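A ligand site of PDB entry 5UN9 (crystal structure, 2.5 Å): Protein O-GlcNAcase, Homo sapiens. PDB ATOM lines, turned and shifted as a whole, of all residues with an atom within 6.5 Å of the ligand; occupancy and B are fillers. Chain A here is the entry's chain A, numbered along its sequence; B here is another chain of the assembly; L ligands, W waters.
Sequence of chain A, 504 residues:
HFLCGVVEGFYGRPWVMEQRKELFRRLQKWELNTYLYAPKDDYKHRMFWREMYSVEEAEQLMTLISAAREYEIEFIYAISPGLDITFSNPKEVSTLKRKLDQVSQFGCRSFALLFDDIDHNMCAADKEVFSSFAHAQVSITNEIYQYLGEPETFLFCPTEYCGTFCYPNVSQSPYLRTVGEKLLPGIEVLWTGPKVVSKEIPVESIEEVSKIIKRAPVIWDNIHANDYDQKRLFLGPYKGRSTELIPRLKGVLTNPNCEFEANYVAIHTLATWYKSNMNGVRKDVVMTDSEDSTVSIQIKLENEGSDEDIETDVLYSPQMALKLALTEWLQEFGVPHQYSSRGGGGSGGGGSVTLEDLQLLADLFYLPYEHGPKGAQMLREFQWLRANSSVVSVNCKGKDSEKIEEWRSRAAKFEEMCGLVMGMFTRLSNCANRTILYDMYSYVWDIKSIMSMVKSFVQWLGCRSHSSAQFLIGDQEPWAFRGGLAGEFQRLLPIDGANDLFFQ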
ATOM      1  N   GLY A   9      14.692 -20.132 -33.677  1.00  0.00           N
ATOM      2  CA  GLY A   9      15.440 -21.009 -32.795  1.00  0.00           C
ATOM      3  C   GLY A   9      14.771 -22.316 -32.396  1.00  0.00           C
ATOM      4  O   GLY A   9      15.032 -22.888 -31.340  1.00  0.00           O
ATOM      5  N   PHE A  10      13.890 -22.796 -33.259  1.00  0.00           N
ATOM      6  CA  PHE A  10      13.045 -23.930 -32.972  1.00  0.00           C
ATOM      7  C   PHE A  10      13.542 -25.189 -33.678  1.00  0.00           C
ATOM      8  O   PHE A  10      14.318 -25.152 -34.634  1.00  0.00           O
ATOM      9  CB  PHE A  10      11.606 -23.618 -33.371  1.00  0.00           C
ATOM     10  CG  PHE A  10      11.475 -23.038 -34.756  1.00  0.00           C
ATOM     11  CD1 PHE A  10      11.586 -23.862 -35.874  1.00  0.00           C
ATOM     12  CD2 PHE A  10      11.216 -21.681 -34.941  1.00  0.00           C
ATOM     13  CE1 PHE A  10      11.457 -23.326 -37.154  1.00  0.00           C
ATOM     14  CE2 PHE A  10      11.080 -21.142 -36.242  1.00  0.00           C
ATOM     15  CZ  PHE A  10      11.204 -21.968 -37.331  1.00  0.00           C
ATOM     16  N   TYR A  11      13.080 -26.309 -33.168  1.00  0.00           N
ATOM     17  CA  TYR A  11      13.352 -27.609 -33.759  1.00  0.00           C
ATOM     18  C   TYR A  11      12.492 -27.844 -34.996  1.00  0.00           C
ATOM     19  O   TYR A  11      11.333 -27.396 -35.068  1.00  0.00           O
ATOM     20  CB  TYR A  11      13.060 -28.700 -32.737  1.00  0.00           C
ATOM     21  CG  TYR A  11      14.040 -28.744 -31.573  1.00  0.00           C
ATOM     22  CD1 TYR A  11      15.215 -29.446 -31.686  1.00  0.00           C
ATOM     23  CD2 TYR A  11      13.745 -28.128 -30.378  1.00  0.00           C
ATOM     24  CE1 TYR A  11      16.102 -29.513 -30.650  1.00  0.00           C
ATOM     25  CE2 TYR A  11      14.614 -28.202 -29.315  1.00  0.00           C
ATOM     26  CZ  TYR A  11      15.805 -28.906 -29.466  1.00  0.00           C
ATOM     27  OH  TYR A  11      16.730 -29.000 -28.430  1.00  0.00           O
ATOM     28  N   ALA A  38      19.221 -19.283 -35.472  1.00  0.00           N
ATOM     29  CA  ALA A  38      19.499 -20.373 -34.546  1.00  0.00           C
ATOM     30  C   ALA A  38      18.610 -21.597 -34.773  1.00  0.00           C
ATOM     31  O   ALA A  38      18.109 -22.152 -33.791  1.00  0.00           O
ATOM     32  CB  ALA A  38      19.337 -19.876 -33.111  1.00  0.00           C
ATOM     33  N   LYS A  40      17.436 -25.123 -34.755  1.00  0.00           N
ATOM     34  CA  LYS A  40      18.084 -26.247 -34.097  1.00  0.00           C
ATOM     35  C   LYS A  40      18.444 -27.360 -35.057  1.00  0.00           C
ATOM     36  O   LYS A  40      19.436 -28.072 -34.851  1.00  0.00           O
ATOM     37  CB  LYS A  40      17.238 -26.826 -32.962  1.00  0.00           C
ATOM     38  CG  LYS A  40      17.205 -25.950 -31.721  1.00  0.00           C
ATOM     39  CD  LYS A  40      18.179 -26.510 -30.656  1.00  0.00           C
ATOM     40  CE  LYS A  40      18.006 -25.777 -29.316  1.00  0.00           C
ATOM     41  NZ  LYS A  40      17.945 -24.261 -29.355  1.00  0.00           N
ATOM     42  N   ASP A 116      22.306 -24.538 -25.000  1.00  0.00           N
ATOM     43  CA  ASP A 116      21.012 -24.996 -24.522  1.00  0.00           C
ATOM     44  C   ASP A 116      20.768 -26.419 -24.981  1.00  0.00           C
ATOM     45  O   ASP A 116      21.316 -26.869 -25.996  1.00  0.00           O
ATOM     46  CB  ASP A 116      19.896 -24.080 -25.037  1.00  0.00           C
ATOM     47  CG  ASP A 116      19.921 -23.933 -26.542  1.00  0.00           C
ATOM     48  OD1 ASP A 116      21.010 -24.036 -27.140  1.00  0.00           O
ATOM     49  OD2 ASP A 116      18.855 -23.693 -27.118  1.00  0.00           O
ATOM     50  N   ASP A 117      19.939 -27.138 -24.210  1.00  0.00           N
ATOM     51  CA  ASP A 117      19.482 -28.479 -24.552  1.00  0.00           C
ATOM     52  C   ASP A 117      20.647 -29.454 -24.791  1.00  0.00           C
ATOM     53  O   ASP A 117      20.716 -30.124 -25.831  1.00  0.00           O
ATOM     54  CB  ASP A 117      18.530 -28.396 -25.755  1.00  0.00           C
ATOM     55  CG  ASP A 117      17.230 -27.657 -25.410  1.00  0.00           C
ATOM     56  OD1 ASP A 117      17.113 -27.235 -24.229  1.00  0.00           O
ATOM     57  OD2 ASP A 117      16.361 -27.468 -26.310  1.00  0.00           O
ATOM     58  N   CYS A 157      24.123 -18.246 -24.552  1.00  0.00           N
ATOM     59  CA  CYS A 157      22.933 -18.893 -23.968  1.00  0.00           C
ATOM     60  C   CYS A 157      23.358 -19.977 -22.992  1.00  0.00           C
ATOM     61  O   CYS A 157      23.975 -20.981 -23.389  1.00  0.00           O
ATOM     62  CB  CYS A 157      22.039 -19.486 -25.062  1.00  0.00           C
ATOM     63  SG  CYS A 157      20.569 -20.235 -24.414  1.00  0.00           S
ATOM     64  N   PRO A 158      23.031 -19.828 -21.718  1.00  0.00           N
ATOM     65  CA  PRO A 158      23.419 -20.841 -20.734  1.00  0.00           C
ATOM     66  C   PRO A 158      22.579 -22.097 -20.881  1.00  0.00           C
ATOM     67  O   PRO A 158      21.461 -22.075 -21.417  1.00  0.00           O
ATOM     68  CB  PRO A 158      23.134 -20.167 -19.402  1.00  0.00           C
ATOM     69  CG  PRO A 158      22.045 -19.118 -19.724  1.00  0.00           C
ATOM     70  CD  PRO A 158      22.194 -18.747 -21.161  1.00  0.00           C
ATOM     71  N   TYR A 161      18.844 -21.996 -18.526  1.00  0.00           N
ATOM     72  CA  TYR A 161      18.330 -20.829 -19.241  1.00  0.00           C
ATOM     73  C   TYR A 161      16.945 -20.389 -18.809  1.00  0.00           C
ATOM     74  O   TYR A 161      16.326 -19.569 -19.505  1.00  0.00           O
ATOM     75  CB  TYR A 161      18.342 -21.081 -20.741  1.00  0.00           C
ATOM     76  CG  TYR A 161      17.526 -22.254 -21.232  1.00  0.00           C
ATOM     77  CD1 TYR A 161      16.103 -22.215 -21.295  1.00  0.00           C
ATOM     78  CD2 TYR A 161      18.171 -23.391 -21.724  1.00  0.00           C
ATOM     79  CE1 TYR A 161      15.360 -23.312 -21.826  1.00  0.00           C
ATOM     80  CE2 TYR A 161      17.453 -24.480 -22.236  1.00  0.00           C
ATOM     81  CZ  TYR A 161      16.065 -24.436 -22.289  1.00  0.00           C
ATOM     82  OH  TYR A 161      15.449 -25.552 -22.801  1.00  0.00           O
ATOM     83  N   LEU A 190      21.201 -14.985 -22.402  1.00  0.00           N
ATOM     84  CA  LEU A 190      19.848 -15.289 -22.872  1.00  0.00           C
ATOM     85  C   LEU A 190      19.084 -16.035 -21.781  1.00  0.00           C
ATOM     86  O   LEU A 190      19.648 -16.871 -21.092  1.00  0.00           O
ATOM     87  CB  LEU A 190      19.914 -16.126 -24.144  1.00  0.00           C
ATOM     88  CG  LEU A 190      20.321 -15.289 -25.365  1.00  0.00           C
ATOM     89  CD1 LEU A 190      20.985 -16.118 -26.477  1.00  0.00           C
ATOM     90  CD2 LEU A 190      19.156 -14.565 -25.920  1.00  0.00           C
ATOM     91  N   TRP A 191      17.795 -15.759 -21.682  1.00  0.00           N
ATOM     92  CA  TRP A 191      16.969 -16.227 -20.563  1.00  0.00           C
ATOM     93  C   TRP A 191      15.553 -16.348 -21.093  1.00  0.00           C
ATOM     94  O   TRP A 191      15.121 -15.473 -21.863  1.00  0.00           O
ATOM     95  CB  TRP A 191      17.029 -15.214 -19.408  1.00  0.00           C
ATOM     96  CG  TRP A 191      16.336 -15.582 -18.148  1.00  0.00           C
ATOM     97  CD1 TRP A 191      15.208 -15.018 -17.662  1.00  0.00           C
ATOM     98  CD2 TRP A 191      16.750 -16.573 -17.186  1.00  0.00           C
ATOM     99  NE1 TRP A 191      14.864 -15.603 -16.455  1.00  0.00           N
ATOM    100  CE2 TRP A 191      15.802 -16.554 -16.143  1.00  0.00           C
ATOM    101  CE3 TRP A 191      17.806 -17.491 -17.120  1.00  0.00           C
ATOM    102  CZ2 TRP A 191      15.890 -17.428 -15.033  1.00  0.00           C
ATOM    103  CZ3 TRP A 191      17.920 -18.347 -15.981  1.00  0.00           C
ATOM    104  CH2 TRP A 191      16.970 -18.297 -14.965  1.00  0.00           C
ATOM    105  N   THR A 192      14.838 -17.432 -20.735  1.00  0.00           N
ATOM    106  CA  THR A 192      13.462 -17.596 -21.241  1.00  0.00           C
ATOM    107  C   THR A 192      12.368 -17.275 -20.208  1.00  0.00           C
ATOM    108  O   THR A 192      11.181 -17.443 -20.518  1.00  0.00           O
ATOM    109  CB  THR A 192      13.173 -19.000 -21.807  1.00  0.00           C
ATOM    110  OG1 THR A 192      13.012 -19.947 -20.750  1.00  0.00           O
ATOM    111  CG2 THR A 192      14.270 -19.489 -22.709  1.00  0.00           C
ATOM    112  N   VAL A 196      10.538 -22.666 -19.496  1.00  0.00           N
ATOM    113  CA  VAL A 196      10.815 -22.734 -20.930  1.00  0.00           C
ATOM    114  C   VAL A 196       9.773 -21.934 -21.703  1.00  0.00           C
ATOM    115  O   VAL A 196      10.126 -21.066 -22.506  1.00  0.00           O
ATOM    116  CB  VAL A 196      10.810 -24.199 -21.404  1.00  0.00           C
ATOM    117  CG1 VAL A 196      11.131 -24.234 -22.901  1.00  0.00           C
ATOM    118  CG2 VAL A 196      11.730 -25.049 -20.531  1.00  0.00           C
ATOM    119  N   VAL A 197       8.491 -22.223 -21.482  1.00  0.00           N
ATOM    120  CA  VAL A 197       7.373 -21.420 -21.981  1.00  0.00           C
ATOM    121  C   VAL A 197       6.781 -20.712 -20.772  1.00  0.00           C
ATOM    122  O   VAL A 197       5.941 -21.247 -20.039  1.00  0.00           O
ATOM    123  CB  VAL A 197       6.310 -22.273 -22.687  1.00  0.00           C
ATOM    124  CG1 VAL A 197       5.142 -21.413 -23.155  1.00  0.00           C
ATOM    125  CG2 VAL A 197       6.911 -23.092 -23.828  1.00  0.00           C
ATOM    126  N   TRP A 220      14.831 -14.614 -24.552  1.00  0.00           N
ATOM    127  CA  TRP A 220      14.421 -15.514 -25.627  1.00  0.00           C
ATOM    128  C   TRP A 220      13.075 -16.052 -25.176  1.00  0.00           C
ATOM    129  O   TRP A 220      12.967 -16.722 -24.154  1.00  0.00           O
ATOM    130  CB  TRP A 220      15.477 -16.607 -25.870  1.00  0.00           C
ATOM    131  CG  TRP A 220      15.145 -17.770 -26.798  1.00  0.00           C
ATOM    132  CD1 TRP A 220      13.962 -18.466 -26.884  1.00  0.00           C
ATOM    133  CD2 TRP A 220      16.050 -18.433 -27.709  1.00  0.00           C
ATOM    134  NE1 TRP A 220      14.072 -19.494 -27.801  1.00  0.00           N
ATOM    135  CE2 TRP A 220      15.349 -19.512 -28.299  1.00  0.00           C
ATOM    136  CE3 TRP A 220      17.382 -18.229 -28.060  1.00  0.00           C
ATOM    137  CZ2 TRP A 220      15.927 -20.358 -29.241  1.00  0.00           C
ATOM    138  CZ3 TRP A 220      17.956 -19.062 -28.975  1.00  0.00           C
ATOM    139  CH2 TRP A 220      17.229 -20.118 -29.574  1.00  0.00           C
ATOM    140  N   ASN A 222       9.544 -18.061 -25.661  1.00  0.00           N
ATOM    141  CA  ASN A 222       8.878 -19.173 -26.351  1.00  0.00           C
ATOM    142  C   ASN A 222       7.348 -19.175 -26.200  1.00  0.00           C
ATOM    143  O   ASN A 222       6.686 -20.173 -26.525  1.00  0.00           O
ATOM    144  CB  ASN A 222       9.475 -20.518 -25.907  1.00  0.00           C
ATOM    145  CG  ASN A 222      10.956 -20.613 -26.136  1.00  0.00           C
ATOM    146  OD1 ASN A 222      11.363 -20.741 -27.296  1.00  0.00           O
ATOM    147  ND2 ASN A 222      11.786 -20.628 -25.062  1.00  0.00           N
ATOM    148  N   ALA A 225       6.066 -20.411 -29.429  1.00  0.00           N
ATOM    149  CA  ALA A 225       6.726 -21.561 -30.006  1.00  0.00           C
ATOM    150  C   ALA A 225       5.738 -22.714 -30.064  1.00  0.00           C
ATOM    151  O   ALA A 225       4.862 -22.837 -29.198  1.00  0.00           O
ATOM    152  CB  ALA A 225       7.940 -21.995 -29.154  1.00  0.00           C
ATOM    153  N   ASN A 226       5.818 -23.523 -31.134  1.00  0.00           N
ATOM    154  CA  ASN A 226       4.866 -24.626 -31.174  1.00  0.00           C
ATOM    155  C   ASN A 226       5.504 -25.900 -31.695  1.00  0.00           C
ATOM    156  O   ASN A 226       4.784 -26.794 -32.152  1.00  0.00           O
ATOM    157  CB  ASN A 226       3.610 -24.256 -31.973  1.00  0.00           C
ATOM    158  CG  ASN A 226       3.841 -24.226 -33.422  1.00  0.00           C
ATOM    159  OD1 ASN A 226       4.988 -24.175 -33.917  1.00  0.00           O
ATOM    160  ND2 ASN A 226       2.744 -24.244 -34.134  1.00  0.00           N
ATOM    161  N   ASP A 227       6.825 -26.007 -31.634  1.00  0.00           N
ATOM    162  CA  ASP A 227       7.531 -27.216 -32.051  1.00  0.00           C
ATOM    163  C   ASP A 227       7.400 -28.368 -31.044  1.00  0.00           C
ATOM    164  O   ASP A 227       7.804 -29.493 -31.352  1.00  0.00           O
ATOM    165  CB  ASP A 227       9.007 -26.870 -32.263  1.00  0.00           C
ATOM    166  CG  ASP A 227       9.688 -26.279 -31.005  1.00  0.00           C
ATOM    167  OD1 ASP A 227       9.030 -26.051 -29.968  1.00  0.00           O
ATOM    168  OD2 ASP A 227      10.898 -26.019 -31.067  1.00  0.00           O
ATOM    169  N   TYR A 228       6.868 -28.130 -29.851  1.00  0.00           N
ATOM    170  CA  TYR A 228       6.851 -29.162 -28.833  1.00  0.00           C
ATOM    171  C   TYR A 228       5.582 -29.990 -28.837  1.00  0.00           C
ATOM    172  O   TYR A 228       5.417 -30.810 -27.932  1.00  0.00           O
ATOM    173  CB  TYR A 228       7.064 -28.563 -27.444  1.00  0.00           C
ATOM    174  CG  TYR A 228       6.138 -27.419 -27.092  1.00  0.00           C
ATOM    175  CD1 TYR A 228       4.783 -27.666 -26.718  1.00  0.00           C
ATOM    176  CD2 TYR A 228       6.605 -26.100 -27.084  1.00  0.00           C
ATOM    177  CE1 TYR A 228       3.921 -26.655 -26.399  1.00  0.00           C
ATOM    178  CE2 TYR A 228       5.743 -25.044 -26.758  1.00  0.00           C
ATOM    179  CZ  TYR A 228       4.399 -25.335 -26.413  1.00  0.00           C
ATOM    180  OH  TYR A 228       3.561 -24.315 -26.076  1.00  0.00           O
ATOM    181  N   ASN A 255      10.811 -16.536 -30.144  1.00  0.00           N
ATOM    182  CA  ASN A 255      10.916 -17.814 -30.837  1.00  0.00           C
ATOM    183  C   ASN A 255       9.505 -18.313 -31.126  1.00  0.00           C
ATOM    184  O   ASN A 255       8.878 -18.845 -30.214  1.00  0.00           O
ATOM    185  CB  ASN A 255      11.625 -18.849 -29.970  1.00  0.00           C
ATOM    186  CG  ASN A 255      11.862 -20.178 -30.683  1.00  0.00           C
ATOM    187  OD1 ASN A 255      12.163 -20.225 -31.872  1.00  0.00           O
ATOM    188  ND2 ASN A 255      11.686 -21.285 -29.939  1.00  0.00           N
ATOM    189  N   TRP B 479       3.834 -28.862 -22.885  1.00  0.00           N
ATOM    190  CA  TRP B 479       3.841 -30.126 -23.606  1.00  0.00           C
ATOM    191  C   TRP B 479       3.420 -31.337 -22.775  1.00  0.00           C
ATOM    192  O   TRP B 479       3.121 -32.377 -23.349  1.00  0.00           O
ATOM    193  CB  TRP B 479       5.222 -30.358 -24.223  1.00  0.00           C
ATOM    194  CG  TRP B 479       6.389 -30.147 -23.283  1.00  0.00           C
ATOM    195  CD1 TRP B 479       6.821 -31.000 -22.313  1.00  0.00           C
ATOM    196  CD2 TRP B 479       7.307 -29.031 -23.269  1.00  0.00           C
ATOM    197  NE1 TRP B 479       7.929 -30.499 -21.690  1.00  0.00           N
ATOM    198  CE2 TRP B 479       8.261 -29.292 -22.250  1.00  0.00           C
ATOM    199  CE3 TRP B 479       7.420 -27.832 -24.001  1.00  0.00           C
ATOM    200  CZ2 TRP B 479       9.314 -28.415 -21.945  1.00  0.00           C
ATOM    201  CZ3 TRP B 479       8.478 -26.964 -23.699  1.00  0.00           C
ATOM    202  CH2 TRP B 479       9.393 -27.258 -22.684  1.00  0.00           C
HETATM  203  C1  LIG L   1      13.656 -24.413 -25.633  1.00  0.00           C
HETATM  204  C2  LIG L   1      14.428 -24.990 -26.832  1.00  0.00           C
HETATM  205  C3  LIG L   1      14.063 -24.218 -28.072  1.00  0.00           C
HETATM  206  C4  LIG L   1      12.719 -24.653 -28.331  1.00  0.00           C
HETATM  207  C5  LIG L   1      11.787 -23.995 -27.259  1.00  0.00           C
HETATM  208  C6  LIG L   1      10.358 -24.415 -27.530  1.00  0.00           C
HETATM  209  C7  LIG L   1      15.904 -23.221 -25.752  1.00  0.00           C
HETATM  210  C8  LIG L   1      17.072 -20.038 -25.129  1.00  0.00           C
HETATM  211  N1  LIG L   1      15.975 -24.372 -26.687  1.00  0.00           N
HETATM  212  O1  LIG L   1      14.840 -24.545 -29.227  1.00  0.00           O
HETATM  213  O2  LIG L   1      12.350 -24.339 -29.666  1.00  0.00           O
HETATM  214  O3  LIG L   1      12.183 -24.460 -25.926  1.00  0.00           O
HETATM  215  N2  LIG L   1      17.026 -22.414 -25.327  1.00  0.00           N
HETATM  216  O4  LIG L   1      10.309 -25.871 -27.615  1.00  0.00           O
HETATM  217  S1  LIG L   1      14.393 -22.990 -25.287  1.00  0.00           S
HETATM  218  C9  LIG L   1      16.743 -21.323 -24.424  1.00  0.00           C
HETATM  219  O   HOH W   1      11.038 -28.051 -26.531  1.00  0.00           O
HETATM  220  O   HOH W   2      14.145 -28.084 -25.357  1.00  0.00           O
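ND2 of Asn 255 lies within hydrogen-bond range of O2 of the ligand, 3.1 Å away. S1 of the ligand sits close to OH of Tyr 161 (3.7 Å). ND2 of Asn 222 lies close to S1 of the ligand (3.5 Å). The side-chain carboxylate of Asp 116 is in hydrogen-bond range of a nitrogen (N2) of the ligand (2.9 Å). O of Gly 9 is in hydrogen-bond range of O1 of the ligand (2.7 Å). The side-chain carboxylate (OD2) of Asp 227 is in hydrogen-bond range of an oxygen (O2) of the ligand. O1 of the ligand sits at hydrogen-bond distance from NZ of Lys 40 (3.1 Å).
The side-chain carboxylate of Asp 117 lies close to a nitrogen (N1) of the ligand. Phe 10 touches the ligand (CA to O2, 3.4 Å). CE2 of Tyr 11 touches O1 of the ligand (3.7 Å). Cys 157 touches the ligand. Thr 192 touches the ligand (CG2 to C9, 3.5 Å). CG1 of Val 196 touches O3 of the ligand, at 3.2 Å. Trp 220 touches the ligand (CD2 to C8, 3.2 Å). CB of Ala 225 touches C6 of the ligand, at 3.8 Å. Tyr 228 touches the ligand (CD2 to O4, 3.7 Å). Hydrophobic or aromatic side chains that line the ligand: Phe 10, Tyr 11, Tyr 161, Val 196, Trp 220, Ala 225 and Tyr 228.
OD1 of Asn 222 lies within hydrogen-bond range of NE1 of Trp 220 (3.0 Å). The backbone carbonyl oxygen (O) of Tyr 161 is in hydrogen-bond range of the backbone NH (N) of Thr 192, at 2.9 Å. The backbone NH (N) of Phe 10 lies within hydrogen-bond range of the side-chain amide oxygen (OD1) of Asn 255, at 3.4 Å. O of Asn 255 lies within hydrogen-bond range of N of Ala 225. The backbone carbonyl oxygen (O) of Trp 191 lies within hydrogen-bond range of the backbone NH (N) of Trp 220, at 2.8 Å. The side-chain amide nitrogen (ND2) of Asn 255 is in hydrogen-bond range of the side-chain amide oxygen (OD1) of Asn 222, 2.7 Å away. N of Gly 9 sits at hydrogen-bond distance from OD1 of Asn 255, at 3.1 Å. OD2 of Asp 227 is in hydrogen-bond range of N of Tyr 11 (3.0 Å).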
